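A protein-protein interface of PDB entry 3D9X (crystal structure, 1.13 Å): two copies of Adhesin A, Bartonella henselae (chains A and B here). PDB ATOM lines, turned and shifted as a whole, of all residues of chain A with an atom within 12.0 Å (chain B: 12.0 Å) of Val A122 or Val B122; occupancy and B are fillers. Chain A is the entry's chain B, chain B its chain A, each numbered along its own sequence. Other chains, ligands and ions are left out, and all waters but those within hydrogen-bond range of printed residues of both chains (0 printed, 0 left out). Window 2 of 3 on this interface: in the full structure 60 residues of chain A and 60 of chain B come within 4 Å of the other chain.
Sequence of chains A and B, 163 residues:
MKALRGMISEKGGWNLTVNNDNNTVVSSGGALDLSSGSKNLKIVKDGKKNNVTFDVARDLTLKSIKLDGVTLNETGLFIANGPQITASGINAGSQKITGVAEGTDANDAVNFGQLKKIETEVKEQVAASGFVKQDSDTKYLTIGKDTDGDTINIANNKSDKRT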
ATOM      1  N   GLY A 113      -2.233 -29.049  -6.854  1.00  0.00           N
ATOM      2  CA  GLY A 113      -2.853 -27.876  -7.485  1.00  0.00           C
ATOM      3  C   GLY A 113      -4.368 -27.879  -7.325  1.00  0.00           C
ATOM      4  O   GLY A 113      -4.975 -26.828  -7.110  1.00  0.00           O
ATOM      5  N   GLN A 114      -5.002 -29.049  -7.412  1.00  0.00           N
ATOM      6  CA  GLN A 114      -6.457 -29.173  -7.218  1.00  0.00           C
ATOM      7  C   GLN A 114      -6.868 -28.877  -5.797  1.00  0.00           C
ATOM      8  O   GLN A 114      -7.873 -28.200  -5.558  1.00  0.00           O
ATOM      9  CB  GLN A 114      -6.944 -30.589  -7.540  1.00  0.00           C
ATOM     10  CG  GLN A 114      -6.804 -30.937  -8.966  1.00  0.00           C
ATOM     11  CD  GLN A 114      -7.327 -32.318  -9.240  1.00  0.00           C
ATOM     12  OE1 GLN A 114      -6.597 -33.308  -9.135  1.00  0.00           O
ATOM     13  NE2 GLN A 114      -8.591 -32.400  -9.635  1.00  0.00           N
ATOM     14  N   LEU A 115      -6.100 -29.390  -4.846  1.00  0.00           N
ATOM     15  CA  LEU A 115      -6.374 -29.150  -3.445  1.00  0.00           C
ATOM     16  C   LEU A 115      -6.240 -27.667  -3.140  1.00  0.00           C
ATOM     17  O   LEU A 115      -7.069 -27.107  -2.421  1.00  0.00           O
ATOM     18  CB  LEU A 115      -5.415 -29.947  -2.564  1.00  0.00           C
ATOM     19  CG  LEU A 115      -5.554 -29.706  -1.061  1.00  0.00           C
ATOM     20  CD1 LEU A 115      -6.945 -30.093  -0.577  1.00  0.00           C
ATOM     21  CD2 LEU A 115      -4.491 -30.479  -0.320  1.00  0.00           C
ATOM     22  N   LYS A 116      -5.203 -27.030  -3.669  1.00  0.00           N
ATOM     23  CA  LYS A 116      -4.981 -25.598  -3.422  1.00  0.00           C
ATOM     24  C   LYS A 116      -6.063 -24.725  -4.054  1.00  0.00           C
ATOM     25  O   LYS A 116      -6.483 -23.720  -3.464  1.00  0.00           O
ATOM     26  CB  LYS A 116      -3.597 -25.172  -3.923  1.00  0.00           C
ATOM     27  CG  LYS A 116      -2.454 -25.717  -3.083  1.00  0.00           C
ATOM     28  CD  LYS A 116      -2.369 -25.043  -1.705  1.00  0.00           C
ATOM     29  CE  LYS A 116      -1.580 -23.744  -1.751  1.00  0.00           C
ATOM     30  NZ  LYS A 116      -0.127 -23.969  -2.004  1.00  0.00           N
ATOM     31  N   LYS A 117      -6.506 -25.109  -5.249  1.00  0.00           N
ATOM     32  CA  LYS A 117      -7.595 -24.422  -5.943  1.00  0.00           C
ATOM     33  C   LYS A 117      -8.840 -24.337  -5.060  1.00  0.00           C
ATOM     34  O   LYS A 117      -9.465 -23.282  -4.956  1.00  0.00           O
ATOM     35  CB  LYS A 117      -7.910 -25.157  -7.249  1.00  0.00           C
ATOM     36  CG  LYS A 117      -9.007 -24.549  -8.106  1.00  0.00           C
ATOM     37  CD  LYS A 117      -9.100 -25.298  -9.426  1.00  0.00           C
ATOM     38  CE  LYS A 117     -10.430 -25.088 -10.124  1.00  0.00           C
ATOM     39  NZ  LYS A 117     -10.484 -25.862 -11.395  1.00  0.00           N
ATOM     40  N   ILE A 118      -9.182 -25.445  -4.408  1.00  0.00           N
ATOM     41  CA  ILE A 118     -10.348 -25.497  -3.521  1.00  0.00           C
ATOM     42  C   ILE A 118     -10.106 -24.734  -2.213  1.00  0.00           C
ATOM     43  O   ILE A 118     -11.039 -24.158  -1.648  1.00  0.00           O
ATOM     44  CB  ILE A 118     -10.766 -26.958  -3.230  1.00  0.00           C
ATOM     45  CG1 ILE A 118     -11.145 -27.660  -4.538  1.00  0.00           C
ATOM     46  CG2 ILE A 118     -11.944 -27.007  -2.264  1.00  0.00           C
ATOM     47  CD1 ILE A 118     -11.711 -29.046  -4.352  1.00  0.00           C
ATOM     48  N   GLU A 119      -8.859 -24.717  -1.744  1.00  0.00           N
ATOM     49  CA  GLU A 119      -8.483 -23.909  -0.580  1.00  0.00           C
ATOM     50  C   GLU A 119      -8.631 -22.416  -0.880  1.00  0.00           C
ATOM     51  O   GLU A 119      -9.078 -21.644  -0.028  1.00  0.00           O
ATOM     52  CB  GLU A 119      -7.043 -24.210  -0.149  1.00  0.00           C
ATOM     53  CG  GLU A 119      -6.684 -23.661   1.227  1.00  0.00           C
ATOM     54  CD  GLU A 119      -5.335 -24.147   1.722  1.00  0.00           C
ATOM     55  OE1 GLU A 119      -4.358 -24.096   0.943  1.00  0.00           O
ATOM     56  OE2 GLU A 119      -5.251 -24.574   2.896  1.00  0.00           O
ATOM     57  N   THR A 120      -8.249 -22.022  -2.094  1.00  0.00           N
ATOM     58  CA  THR A 120      -8.333 -20.630  -2.534  1.00  0.00           C
ATOM     59  C   THR A 120      -9.778 -20.170  -2.735  1.00  0.00           C
ATOM     60  O   THR A 120     -10.132 -19.047  -2.364  1.00  0.00           O
ATOM     61  CB  THR A 120      -7.566 -20.420  -3.854  1.00  0.00           C
ATOM     62  OG1 THR A 120      -6.215 -20.873  -3.702  1.00  0.00           O
ATOM     63  CG2 THR A 120      -7.566 -18.948  -4.257  1.00  0.00           C
ATOM     64  N   GLU A 121     -10.602 -21.037  -3.324  1.00  0.00           N
ATOM     65  CA  GLU A 121     -12.001 -20.711  -3.630  1.00  0.00           C
ATOM     66  C   GLU A 121     -12.828 -20.351  -2.391  1.00  0.00           C
ATOM     67  O   GLU A 121     -13.738 -19.521  -2.473  1.00  0.00           O
ATOM     68  CB  GLU A 121     -12.669 -21.866  -4.392  1.00  0.00           C
ATOM     69  CG  GLU A 121     -12.295 -21.928  -5.874  1.00  0.00           C
ATOM     70  CD  GLU A 121     -12.746 -23.213  -6.557  1.00  0.00           C
ATOM     71  OE1 GLU A 121     -13.538 -23.973  -5.959  1.00  0.00           O
ATOM     72  OE2 GLU A 121     -12.307 -23.461  -7.702  1.00  0.00           O
ATOM     73  N   VAL A 122     -12.515 -20.969  -1.254  1.00  0.00           N
ATOM     74  CA  VAL A 122     -13.220 -20.677  -0.003  1.00  0.00           C
ATOM     75  C   VAL A 122     -12.614 -19.453   0.679  1.00  0.00           C
ATOM     76  O   VAL A 122     -13.095 -18.333   0.503  1.00  0.00           O
ATOM     77  CB  VAL A 122     -13.193 -21.879   0.969  1.00  0.00           C
ATOM     78  CG1 VAL A 122     -11.781 -22.129   1.487  1.00  0.00           C
ATOM     79  CG2 VAL A 122     -14.158 -21.650   2.124  1.00  0.00           C
ATOM     80  N   PHE B 112     -10.570 -38.253  -6.233  1.00  0.00           N
ATOM     81  CA  PHE B 112     -11.290 -37.035  -6.556  1.00  0.00           C
ATOM     82  C   PHE B 112     -12.662 -36.994  -5.886  1.00  0.00           C
ATOM     83  O   PHE B 112     -13.115 -35.940  -5.447  1.00  0.00           O
ATOM     84  CB  PHE B 112     -11.407 -36.940  -8.074  1.00  0.00           C
ATOM     85  CG  PHE B 112     -12.069 -35.688  -8.566  1.00  0.00           C
ATOM     86  CD1 PHE B 112     -11.440 -34.465  -8.472  1.00  0.00           C
ATOM     87  CD2 PHE B 112     -13.310 -35.747  -9.169  1.00  0.00           C
ATOM     88  CE1 PHE B 112     -12.052 -33.312  -8.948  1.00  0.00           C
ATOM     89  CE2 PHE B 112     -13.926 -34.589  -9.649  1.00  0.00           C
ATOM     90  CZ  PHE B 112     -13.286 -33.386  -9.537  1.00  0.00           C
ATOM     91  N   GLY B 113     -13.316 -38.136  -5.762  1.00  0.00           N
ATOM     92  CA  GLY B 113     -14.560 -38.188  -5.004  1.00  0.00           C
ATOM     93  C   GLY B 113     -14.391 -37.676  -3.579  1.00  0.00           C
ATOM     94  O   GLY B 113     -15.279 -37.024  -3.044  1.00  0.00           O
ATOM     95  N   GLN B 114     -13.264 -37.974  -2.941  1.00  0.00           N
ATOM     96  CA  GLN B 114     -12.981 -37.474  -1.576  1.00  0.00           C
ATOM     97  C   GLN B 114     -12.758 -35.976  -1.532  1.00  0.00           C
ATOM     98  O   GLN B 114     -13.202 -35.309  -0.597  1.00  0.00           O
ATOM     99  CB  GLN B 114     -11.737 -38.148  -0.998  1.00  0.00           C
ATOM    100  CG  GLN B 114     -11.895 -39.626  -0.765  1.00  0.00           C
ATOM    101  CD  GLN B 114     -10.653 -40.242  -0.142  1.00  0.00           C
ATOM    102  OE1 GLN B 114      -9.732 -40.603  -0.844  1.00  0.00           O
ATOM    103  NE2 GLN B 114     -10.644 -40.388   1.179  1.00  0.00           N
ATOM    104  N   LEU B 115     -12.037 -35.452  -2.511  1.00  0.00           N
ATOM    105  CA  LEU B 115     -11.780 -34.022  -2.597  1.00  0.00           C
ATOM    106  C   LEU B 115     -13.077 -33.245  -2.778  1.00  0.00           C
ATOM    107  O   LEU B 115     -13.271 -32.204  -2.135  1.00  0.00           O
ATOM    108  CB  LEU B 115     -10.836 -33.713  -3.756  1.00  0.00           C
ATOM    109  CG  LEU B 115     -10.422 -32.248  -3.913  1.00  0.00           C
ATOM    110  CD1 LEU B 115      -9.438 -31.849  -2.828  1.00  0.00           C
ATOM    111  CD2 LEU B 115      -9.829 -32.029  -5.282  1.00  0.00           C
ATOM    112  N   LYS B 116     -13.967 -33.749  -3.634  1.00  0.00           N
ATOM    113  CA  LYS B 116     -15.229 -33.059  -3.933  1.00  0.00           C
ATOM    114  C   LYS B 116     -16.184 -33.069  -2.743  1.00  0.00           C
ATOM    115  O   LYS B 116     -16.978 -32.140  -2.568  1.00  0.00           O
ATOM    116  CB  LYS B 116     -15.907 -33.674  -5.165  1.00  0.00           C
ATOM    117  CG  LYS B 116     -15.115 -33.510  -6.454  1.00  0.00           C
ATOM    118  CD  LYS B 116     -15.125 -32.070  -6.967  1.00  0.00           C
ATOM    119  CE  LYS B 116     -16.417 -31.729  -7.689  1.00  0.00           C
ATOM    120  NZ  LYS B 116     -16.281 -30.492  -8.509  1.00  0.00           N
ATOM    121  N   LYS B 117     -16.112 -34.119  -1.930  1.00  0.00           N
ATOM    122  CA  LYS B 117     -16.910 -34.191  -0.707  1.00  0.00           C
ATOM    123  C   LYS B 117     -16.494 -33.081   0.262  1.00  0.00           C
ATOM    124  O   LYS B 117     -17.348 -32.383   0.816  1.00  0.00           O
ATOM    125  CB  LYS B 117     -16.757 -35.566  -0.053  1.00  0.00           C
ATOM    126  CG  LYS B 117     -17.651 -35.780   1.159  1.00  0.00           C
ATOM    127  CD  LYS B 117     -17.486 -37.178   1.746  1.00  0.00           C
ATOM    128  CE  LYS B 117     -16.208 -37.315   2.563  1.00  0.00           C
ATOM    129  NZ  LYS B 117     -16.197 -36.459   3.783  1.00  0.00           N
ATOM    130  N   ILE B 118     -15.187 -32.902   0.445  1.00  0.00           N
ATOM    131  CA  ILE B 118     -14.660 -31.865   1.342  1.00  0.00           C
ATOM    132  C   ILE B 118     -14.924 -30.459   0.803  1.00  0.00           C
ATOM    133  O   ILE B 118     -15.157 -29.530   1.581  1.00  0.00           O
ATOM    134  CB  ILE B 118     -13.142 -32.042   1.595  1.00  0.00           C
ATOM    135  CG1 ILE B 118     -12.862 -33.389   2.263  1.00  0.00           C
ATOM    136  CG2 ILE B 118     -12.599 -30.923   2.475  1.00  0.00           C
ATOM    137  CD1 ILE B 118     -13.592 -33.608   3.573  1.00  0.00           C
ATOM    138  N   GLU B 119     -14.886 -30.307  -0.520  1.00  0.00           N
ATOM    139  CA  GLU B 119     -15.219 -29.037  -1.167  1.00  0.00           C
ATOM    140  C   GLU B 119     -16.659 -28.631  -0.864  1.00  0.00           C
ATOM    141  O   GLU B 119     -16.918 -27.497  -0.455  1.00  0.00           O
ATOM    142  CB  GLU B 119     -15.019 -29.135  -2.682  1.00  0.00           C
ATOM    143  CG  GLU B 119     -15.251 -27.823  -3.432  1.00  0.00           C
ATOM    144  CD  GLU B 119     -15.114 -27.961  -4.938  1.00  0.00           C
ATOM    145  OE1 GLU B 119     -14.738 -29.051  -5.417  1.00  0.00           O
ATOM    146  OE2 GLU B 119     -15.387 -26.967  -5.648  1.00  0.00           O
ATOM    147  N   THR B 120     -17.587 -29.562  -1.070  1.00  0.00           N
ATOM    148  CA  THR B 120     -19.005 -29.321  -0.805  1.00  0.00           C
ATOM    149  C   THR B 120     -19.267 -29.046   0.678  1.00  0.00           C
ATOM    150  O   THR B 120     -20.170 -28.279   1.020  1.00  0.00           O
ATOM    151  CB  THR B 120     -19.867 -30.512  -1.268  1.00  0.00           C
ATOM    152  OG1 THR B 120     -19.580 -30.801  -2.641  1.00  0.00           O
ATOM    153  CG2 THR B 120     -21.353 -30.205  -1.114  1.00  0.00           C
ATOM    154  N   GLU B 121     -18.479 -29.670   1.551  1.00  0.00           N
ATOM    155  CA  GLU B 121     -18.567 -29.413   2.990  1.00  0.00           C
ATOM    156  C   GLU B 121     -18.054 -28.013   3.333  1.00  0.00           C
ATOM    157  O   GLU B 121     -18.781 -27.214   3.925  1.00  0.00           O
ATOM    158  CB  GLU B 121     -17.785 -30.466   3.782  1.00  0.00           C
ATOM    159  CG  GLU B 121     -18.464 -31.829   3.839  1.00  0.00           C
ATOM    160  CD  GLU B 121     -17.584 -32.901   4.459  1.00  0.00           C
ATOM    161  OE1 GLU B 121     -16.684 -32.555   5.253  1.00  0.00           O
ATOM    162  OE2 GLU B 121     -17.798 -34.095   4.157  1.00  0.00           O
ATOM    163  N   VAL B 122     -16.816 -27.719   2.940  1.00  0.00           N
ATOM    164  CA  VAL B 122     -16.167 -26.439   3.266  1.00  0.00           C
ATOM    165  C   VAL B 122     -16.971 -25.211   2.815  1.00  0.00           C
ATOM    166  O   VAL B 122     -16.904 -24.156   3.452  1.00  0.00           O
ATOM    167  CB  VAL B 122     -14.727 -26.360   2.681  1.00  0.00           C
ATOM    168  CG1 VAL B 122     -14.758 -26.214   1.167  1.00  0.00           C
ATOM    169  CG2 VAL B 122     -13.953 -25.210   3.312  1.00  0.00           C
ATOM    170  N   LYS B 123     -17.729 -25.352   1.728  1.00  0.00           N
ATOM    171  CA  LYS B 123     -18.572 -24.266   1.217  1.00  0.00           C
ATOM    172  C   LYS B 123     -19.788 -23.955   2.101  1.00  0.00           C
ATOM    173  O   LYS B 123     -20.418 -22.910   1.931  1.00  0.00           O
ATOM    174  CB  LYS B 123     -19.033 -24.574  -0.213  1.00  0.00           C
ATOM    175  CG  LYS B 123     -17.929 -24.441  -1.248  1.00  0.00           C
ATOM    176  CD  LYS B 123     -18.363 -24.980  -2.599  1.00  0.00           C
ATOM    177  CE  LYS B 123     -17.286 -24.772  -3.650  1.00  0.00           C
ATOM    178  NZ  LYS B 123     -17.633 -25.435  -4.937  1.00  0.00           N
ATOM    179  N   GLU B 124     -20.126 -24.860   3.023  1.00  0.00           N
ATOM    180  CA  GLU B 124     -21.188 -24.610   4.007  1.00  0.00           C
ATOM    181  C   GLU B 124     -20.809 -25.036   5.437  1.00  0.00           C
ATOM    182  O   GLU B 124     -21.686 -25.198   6.290  1.00  0.00           O
ATOM    183  CB  GLU B 124     -22.485 -25.309   3.574  1.00  0.00           C
ATOM    184  CG  GLU B 124     -22.384 -26.830   3.471  1.00  0.00           C
ATOM    185  CD  GLU B 124     -23.708 -27.487   3.105  1.00  0.00           C
ATOM    186  OE1 GLU B 124     -23.708 -28.384   2.234  1.00  0.00           O
ATOM    187  OE2 GLU B 124     -24.749 -27.109   3.685  1.00  0.00           O
ATOM    188  N   GLN B 125     -19.510 -25.194   5.697  1.00  0.00           N
ATOM    189  CA  GLN B 125     -19.014 -25.632   7.006  1.00  0.00           C
ATOM    190  C   GLN B 125     -18.167 -24.537   7.644  1.00  0.00           C
ATOM    191  O   GLN B 125     -17.333 -23.919   6.984  1.00  0.00           O
ATOM    192  CB  GLN B 125     -18.192 -26.916   6.856  1.00  0.00           C
ATOM    193  CG  GLN B 125     -17.695 -27.523   8.161  1.00  0.00           C
ATOM    194  CD  GLN B 125     -17.056 -28.888   7.959  1.00  0.00           C
ATOM    195  OE1 GLN B 125     -15.860 -29.069   8.191  1.00  0.00           O
ATOM    196  NE2 GLN B 125     -17.854 -29.854   7.515  1.00  0.00           N
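Leu A115 touches its own counterpart, Leu B115. Ile A118 touches Leu B115, but with the chains exchanged Leu A115 does not touch Ile B118 (6.5 Å). Ile A118 touches Glu B119, but with the chains exchanged Glu A119 does not touch Ile B118 (8.4 Å). Glu A121 touches Glu B119, but with the chains exchanged Glu A119 does not touch Glu B121 (11.0 Å). 10 positions are printed for both chains.
NZ of Lys B116 lies within salt-bridge range of OE1 of Glu B119 (3.7 Å). The side-chain amino group (NZ) of Lys B123 lies within salt-bridge range of the side-chain carboxylate (OE2) of Glu B119.
Printed residues of chain A that touch a printed residue of chain B: Gln A114, Leu A115, Ile A118, Glu A121 and Val A122. Hydrophobic or aromatic side chains of chain A within 4 Å of the printed part of chain B: Leu A115, Ile A118 and Val A122. Printed residues of chain B that touch a printed residue of chain A: Phe B112, Leu B115, Glu B119 and Val B122. Among the printed residues, 7 pairs touch across the chains.
Phe B112 touches Gln A114 (CE1 to NE2, 3.6 Å). Leu B115 touches Gln A114 (CD2 to CB, 3.9 Å). Leu A115 touches Leu B115. CD1 of Ile A118 touches CG of Leu B115, 3.5 Å away. Ile A118 touches Glu B119. OE2 of Glu B119 touches OE1 of Glu A121, 3.5 Å away. CG2 of Val A122 touches CG2 of Val B122, at 3.8 Å.
Printed residues of chain B within 4 Å of Leu A115: Leu B115 (3.8 Å). Of chain B, only Leu B115 (3.5 Å) and Glu B119 (3.2 Å) come within 4 Å of Ile A118. No residue of chain B comes within 4 Å of Glu A119. No residue of chain B comes within 4 Å of Thr A120. Of chain B, only Glu B119 (3.5 Å) comes within 4 Å of Glu A121. Gln B114 touches none of the printed residues of chain A. Printed residues of chain A within 4 Å of Leu B115: Gln A114, Leu A115 and Ile A118. No residue of chain A comes within 4 Å of Ile B118. No residue of chain A comes within 4 Å of Thr B120. No residue of chain A comes within 4 Å of Gln B125. The nearest residue of chain B that does not touch Val A122 is Lys B123 (5.2 Å). The nearest printed residue of chain B that does not touch Leu A115 is Ile B118 (6.5 Å).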
